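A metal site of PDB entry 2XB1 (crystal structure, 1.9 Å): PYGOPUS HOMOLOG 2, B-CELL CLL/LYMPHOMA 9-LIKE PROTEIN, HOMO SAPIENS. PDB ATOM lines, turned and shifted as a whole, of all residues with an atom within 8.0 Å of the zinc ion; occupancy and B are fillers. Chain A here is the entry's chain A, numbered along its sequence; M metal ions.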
ATOM      1  N   GLY A   7       8.907 -21.225  -2.091  1.00  0.00           N
ATOM      2  CA  GLY A   7      10.076 -21.893  -2.631  1.00  0.00           C
ATOM      3  C   GLY A   7      11.300 -21.007  -2.783  1.00  0.00           C
ATOM      4  O   GLY A   7      12.414 -21.516  -2.970  1.00  0.00           O
ATOM      5  N   LEU A  21       2.193 -22.262  -8.214  1.00  0.00           N
ATOM      6  CA  LEU A  21       2.662 -23.543  -7.707  1.00  0.00           C
ATOM      7  C   LEU A  21       3.523 -24.191  -8.775  1.00  0.00           C
ATOM      8  O   LEU A  21       3.087 -24.308  -9.919  1.00  0.00           O
ATOM      9  CB  LEU A  21       1.437 -24.401  -7.446  1.00  0.00           C
ATOM     10  CG  LEU A  21       1.758 -25.875  -7.177  1.00  0.00           C
ATOM     11  CD1 LEU A  21       2.612 -26.081  -5.896  1.00  0.00           C
ATOM     12  CD2 LEU A  21       0.377 -26.640  -7.046  1.00  0.00           C
ATOM     13  N   CYS A  22       4.703 -24.666  -8.412  1.00  0.00           N
ATOM     14  CA  CYS A  22       5.467 -25.502  -9.411  1.00  0.00           C
ATOM     15  C   CYS A  22       4.885 -26.963  -9.409  1.00  0.00           C
ATOM     16  O   CYS A  22       5.429 -27.908  -8.839  1.00  0.00           O
ATOM     17  CB  CYS A  22       7.003 -25.437  -9.106  1.00  0.00           C
ATOM     18  SG  CYS A  22       8.049 -26.319 -10.388  1.00  0.00           S
ATOM     19  N   GLU A  23       3.773 -27.163 -10.074  1.00  0.00           N
ATOM     20  CA  GLU A  23       2.961 -28.346  -9.713  1.00  0.00           C
ATOM     21  C   GLU A  23       3.410 -29.597 -10.409  1.00  0.00           C
ATOM     22  O   GLU A  23       3.029 -30.729  -9.967  1.00  0.00           O
ATOM     23  CB  GLU A  23       1.466 -28.134  -9.981  1.00  0.00           C
ATOM     24  CG  GLU A  23       1.136 -27.733 -11.387  1.00  0.00           C
ATOM     25  CD  GLU A  23      -0.318 -27.327 -11.511  1.00  0.00           C
ATOM     26  OE1 GLU A  23      -1.234 -28.162 -11.173  1.00  0.00           O
ATOM     27  OE2 GLU A  23      -0.527 -26.169 -11.953  1.00  0.00           O
ATOM     28  N   ALA A  24       4.170 -29.421 -11.505  1.00  0.00           N
ATOM     29  CA  ALA A  24       4.583 -30.567 -12.293  1.00  0.00           C
ATOM     30  C   ALA A  24       5.982 -31.045 -11.892  1.00  0.00           C
ATOM     31  O   ALA A  24       6.534 -31.988 -12.520  1.00  0.00           O
ATOM     32  CB  ALA A  24       4.527 -30.233 -13.764  1.00  0.00           C
ATOM     33  N   SER A  25       6.543 -30.405 -10.853  1.00  0.00           N
ATOM     34  CA  SER A  25       7.894 -30.718 -10.482  1.00  0.00           C
ATOM     35  C   SER A  25       8.122 -30.680  -8.957  1.00  0.00           C
ATOM     36  O   SER A  25       7.786 -31.624  -8.236  1.00  0.00           O
ATOM     37  CB  SER A  25       8.883 -29.768 -11.171  1.00  0.00           C
ATOM     38  OG  SER A  25      10.153 -30.436 -11.184  1.00  0.00           O
ATOM     39  N   CYS A  26       8.609 -29.547  -8.461  1.00  0.00           N
ATOM     40  CA  CYS A  26       9.123 -29.513  -7.082  1.00  0.00           C
ATOM     41  C   CYS A  26       8.040 -29.352  -6.014  1.00  0.00           C
ATOM     42  O   CYS A  26       8.312 -29.496  -4.822  1.00  0.00           O
ATOM     43  CB  CYS A  26      10.228 -28.441  -6.872  1.00  0.00           C
ATOM     44  SG  CYS A  26       9.643 -26.713  -6.785  1.00  0.00           S
ATOM     45  N   GLN A  27       6.818 -29.053  -6.448  1.00  0.00           N
ATOM     46  CA  GLN A  27       5.671 -29.014  -5.554  1.00  0.00           C
ATOM     47  C   GLN A  27       5.709 -27.904  -4.471  1.00  0.00           C
ATOM     48  O   GLN A  27       5.139 -28.065  -3.364  1.00  0.00           O
ATOM     49  CB  GLN A  27       5.379 -30.427  -4.962  1.00  0.00           C
ATOM     50  CG  GLN A  27       5.016 -31.424  -6.098  1.00  0.00           C
ATOM     51  CD  GLN A  27       4.498 -32.764  -5.546  1.00  0.00           C
ATOM     52  OE1 GLN A  27       5.219 -33.441  -4.810  1.00  0.00           O
ATOM     53  NE2 GLN A  27       3.251 -33.136  -5.893  1.00  0.00           N
ATOM     54  N   LYS A  28       6.412 -26.806  -4.776  1.00  0.00           N
ATOM     55  CA  LYS A  28       6.464 -25.688  -3.842  1.00  0.00           C
ATOM     56  C   LYS A  28       5.617 -24.541  -4.443  1.00  0.00           C
ATOM     57  O   LYS A  28       5.679 -24.299  -5.664  1.00  0.00           O
ATOM     58  CB  LYS A  28       7.897 -25.205  -3.661  1.00  0.00           C
ATOM     59  CG  LYS A  28       8.857 -26.270  -3.036  1.00  0.00           C
ATOM     60  CD  LYS A  28      10.282 -25.779  -3.068  1.00  0.00           C
ATOM     61  CE  LYS A  28      11.224 -26.929  -2.656  1.00  0.00           C
ATOM     62  NZ  LYS A  28      12.600 -26.473  -2.876  1.00  0.00           N
ATOM     63  N   TRP A  29       4.864 -23.876  -3.557  1.00  0.00           N
ATOM     64  CA  TRP A  29       4.251 -22.579  -3.831  1.00  0.00           C
ATOM     65  C   TRP A  29       5.289 -21.444  -3.802  1.00  0.00           C
ATOM     66  O   TRP A  29       6.278 -21.562  -3.080  1.00  0.00           O
ATOM     67  CB  TRP A  29       3.144 -22.298  -2.789  1.00  0.00           C
ATOM     68  CG  TRP A  29       1.926 -23.087  -3.077  1.00  0.00           C
ATOM     69  CD1 TRP A  29       1.580 -24.337  -2.537  1.00  0.00           C
ATOM     70  CD2 TRP A  29       0.860 -22.730  -3.951  1.00  0.00           C
ATOM     71  NE1 TRP A  29       0.366 -24.760  -3.057  1.00  0.00           N
ATOM     72  CE2 TRP A  29      -0.104 -23.791  -3.909  1.00  0.00           C
ATOM     73  CE3 TRP A  29       0.613 -21.622  -4.795  1.00  0.00           C
ATOM     74  CZ2 TRP A  29      -1.282 -23.760  -4.662  1.00  0.00           C
ATOM     75  CZ3 TRP A  29      -0.559 -21.588  -5.541  1.00  0.00           C
ATOM     76  CH2 TRP A  29      -1.495 -22.654  -5.477  1.00  0.00           C
ATOM     77  N   PHE A  30       5.087 -20.382  -4.578  1.00  0.00           N
ATOM     78  CA  PHE A  30       6.015 -19.224  -4.613  1.00  0.00           C
ATOM     79  C   PHE A  30       5.133 -17.985  -4.577  1.00  0.00           C
ATOM     80  O   PHE A  30       4.180 -17.874  -5.362  1.00  0.00           O
ATOM     81  CB  PHE A  30       6.844 -19.169  -5.930  1.00  0.00           C
ATOM     82  CG  PHE A  30       7.938 -20.221  -6.041  1.00  0.00           C
ATOM     83  CD1 PHE A  30       9.287 -19.874  -5.879  1.00  0.00           C
ATOM     84  CD2 PHE A  30       7.624 -21.556  -6.273  1.00  0.00           C
ATOM     85  CE1 PHE A  30      10.305 -20.844  -6.013  1.00  0.00           C
ATOM     86  CE2 PHE A  30       8.630 -22.550  -6.373  1.00  0.00           C
ATOM     87  CZ  PHE A  30       9.951 -22.206  -6.269  1.00  0.00           C
ATOM     88  N   TRP A  53       3.170 -23.932 -14.648  1.00  0.00           N
ATOM     89  CA  TRP A  53       4.377 -23.105 -14.478  1.00  0.00           C
ATOM     90  C   TRP A  53       5.532 -23.985 -13.914  1.00  0.00           C
ATOM     91  O   TRP A  53       5.308 -24.895 -13.040  1.00  0.00           O
ATOM     92  CB  TRP A  53       4.059 -21.937 -13.530  1.00  0.00           C
ATOM     93  CG  TRP A  53       5.240 -21.093 -13.161  1.00  0.00           C
ATOM     94  CD1 TRP A  53       5.925 -20.171 -13.985  1.00  0.00           C
ATOM     95  CD2 TRP A  53       5.889 -21.064 -11.893  1.00  0.00           C
ATOM     96  NE1 TRP A  53       6.967 -19.615 -13.279  1.00  0.00           N
ATOM     97  CE2 TRP A  53       6.972 -20.147 -11.995  1.00  0.00           C
ATOM     98  CE3 TRP A  53       5.672 -21.731 -10.673  1.00  0.00           C
ATOM     99  CZ2 TRP A  53       7.821 -19.859 -10.895  1.00  0.00           C
ATOM    100  CZ3 TRP A  53       6.521 -21.443  -9.573  1.00  0.00           C
ATOM    101  CH2 TRP A  53       7.593 -20.508  -9.701  1.00  0.00           C
ATOM    102  N   ALA A  54       6.737 -23.724 -14.393  1.00  0.00           N
ATOM    103  CA  ALA A  54       7.956 -24.322 -13.812  1.00  0.00           C
ATOM    104  C   ALA A  54       8.881 -23.235 -13.207  1.00  0.00           C
ATOM    105  O   ALA A  54       9.151 -22.194 -13.872  1.00  0.00           O
ATOM    106  CB  ALA A  54       8.698 -25.145 -14.868  1.00  0.00           C
ATOM    107  N   CYS A  55       9.338 -23.470 -11.963  1.00  0.00           N
ATOM    108  CA  CYS A  55      10.187 -22.470 -11.260  1.00  0.00           C
ATOM    109  C   CYS A  55      11.623 -22.494 -11.815  1.00  0.00           C
ATOM    110  O   CYS A  55      12.009 -23.402 -12.563  1.00  0.00           O
ATOM    111  CB  CYS A  55      10.195 -22.693  -9.753  1.00  0.00           C
ATOM    112  SG  CYS A  55      11.291 -24.137  -9.221  1.00  0.00           S
ATOM    113  N   ASP A  56      12.397 -21.489 -11.446  1.00  0.00           N
ATOM    114  CA  ASP A  56      13.760 -21.318 -12.001  1.00  0.00           C
ATOM    115  C   ASP A  56      14.695 -22.429 -11.522  1.00  0.00           C
ATOM    116  O   ASP A  56      15.592 -22.823 -12.271  1.00  0.00           O
ATOM    117  CB  ASP A  56      14.377 -20.040 -11.498  1.00  0.00           C
ATOM    118  CG  ASP A  56      13.654 -18.799 -11.970  1.00  0.00           C
ATOM    119  OD1 ASP A  56      12.756 -18.853 -12.825  1.00  0.00           O
ATOM    120  OD2 ASP A  56      14.043 -17.725 -11.481  1.00  0.00           O
ATOM    121  N   LEU A  57      14.481 -22.933 -10.289  1.00  0.00           N
ATOM    122  CA  LEU A  57      15.409 -23.963  -9.790  1.00  0.00           C
ATOM    123  C   LEU A  57      15.143 -25.316 -10.506  1.00  0.00           C
ATOM    124  O   LEU A  57      16.084 -26.019 -10.818  1.00  0.00           O
ATOM    125  CB  LEU A  57      15.346 -24.141  -8.252  1.00  0.00           C
ATOM    126  CG  LEU A  57      16.379 -25.081  -7.581  1.00  0.00           C
ATOM    127  CD1 LEU A  57      17.867 -24.837  -8.036  1.00  0.00           C
ATOM    128  CD2 LEU A  57      16.250 -25.138  -5.984  1.00  0.00           C
ATOM    129  N   CYS A  58      13.882 -25.669 -10.731  1.00  0.00           N
ATOM    130  CA  CYS A  58      13.569 -26.825 -11.559  1.00  0.00           C
ATOM    131  C   CYS A  58      14.104 -26.668 -12.986  1.00  0.00           C
ATOM    132  O   CYS A  58      14.632 -27.657 -13.561  1.00  0.00           O
ATOM    133  CB  CYS A  58      12.060 -27.091 -11.546  1.00  0.00           C
ATOM    134  SG  CYS A  58      11.548 -27.779  -9.921  1.00  0.00           S
ATOM    135  N   LEU A  59      14.012 -25.477 -13.558  1.00  0.00           N
ATOM    136  CA  LEU A  59      14.510 -25.278 -14.911  1.00  0.00           C
ATOM    137  C   LEU A  59      16.039 -25.506 -14.942  1.00  0.00           C
ATOM    138  O   LEU A  59      16.567 -26.136 -15.850  1.00  0.00           O
ATOM    139  CB  LEU A  59      14.182 -23.872 -15.357  1.00  0.00           C
ATOM    140  CG  LEU A  59      14.825 -23.409 -16.636  1.00  0.00           C
ATOM    141  CD1 LEU A  59      14.117 -24.148 -17.799  1.00  0.00           C
ATOM    142  CD2 LEU A  59      14.598 -21.909 -16.654  1.00  0.00           C
ATOM    143  N   GLU A  63      14.509 -30.528 -13.999  1.00  0.00           N
ATOM    144  CA  GLU A  63      13.708 -31.425 -13.168  1.00  0.00           C
ATOM    145  C   GLU A  63      12.452 -31.912 -13.921  1.00  0.00           C
ATOM    146  O   GLU A  63      11.804 -31.134 -14.628  1.00  0.00           O
ATOM    147  CB  GLU A  63      13.282 -30.721 -11.876  1.00  0.00           C
ATOM    148  CG  GLU A  63      14.211 -30.842 -10.666  1.00  0.00           C
ATOM    149  CD  GLU A  63      14.547 -32.288 -10.273  1.00  0.00           C
ATOM    150  OE1 GLU A  63      14.047 -32.791  -9.229  1.00  0.00           O
ATOM    151  OE2 GLU A  63      15.315 -32.927 -11.023  1.00  0.00           O
HETATM  152 ZN    ZN M   1      10.081 -26.157  -9.082  1.00  0.00          ZN
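N of Leu 57 sits close to SG of Cys 55, at 3.6 Å.
The backbone carbonyl oxygen of Cys 22 sits at hydrogen-bond distance from the backbone NH of Gln 27 (3.0 Å).
The backbone NH (N) of Cys 22 lies within hydrogen-bond range of the backbone carbonyl oxygen (O) of Lys 28 (2.9 Å).
The side-chain sulfur of Cys 58 sits close to the side-chain hydroxyl of Ser 25 (3.3 Å).
N of Glu 63 sits at hydrogen-bond distance from O of Cys 58, 2.9 Å away.
Of the 19 residues printed, 4 come within 4 Å of the zinc ion.
The zinc ion is bound by SG of Cys 58 (2.3 Å), SG of Cys 55 (2.4 Å), SG of Cys 26 (2.4 Å) and SG of Cys 22 (2.4 Å).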
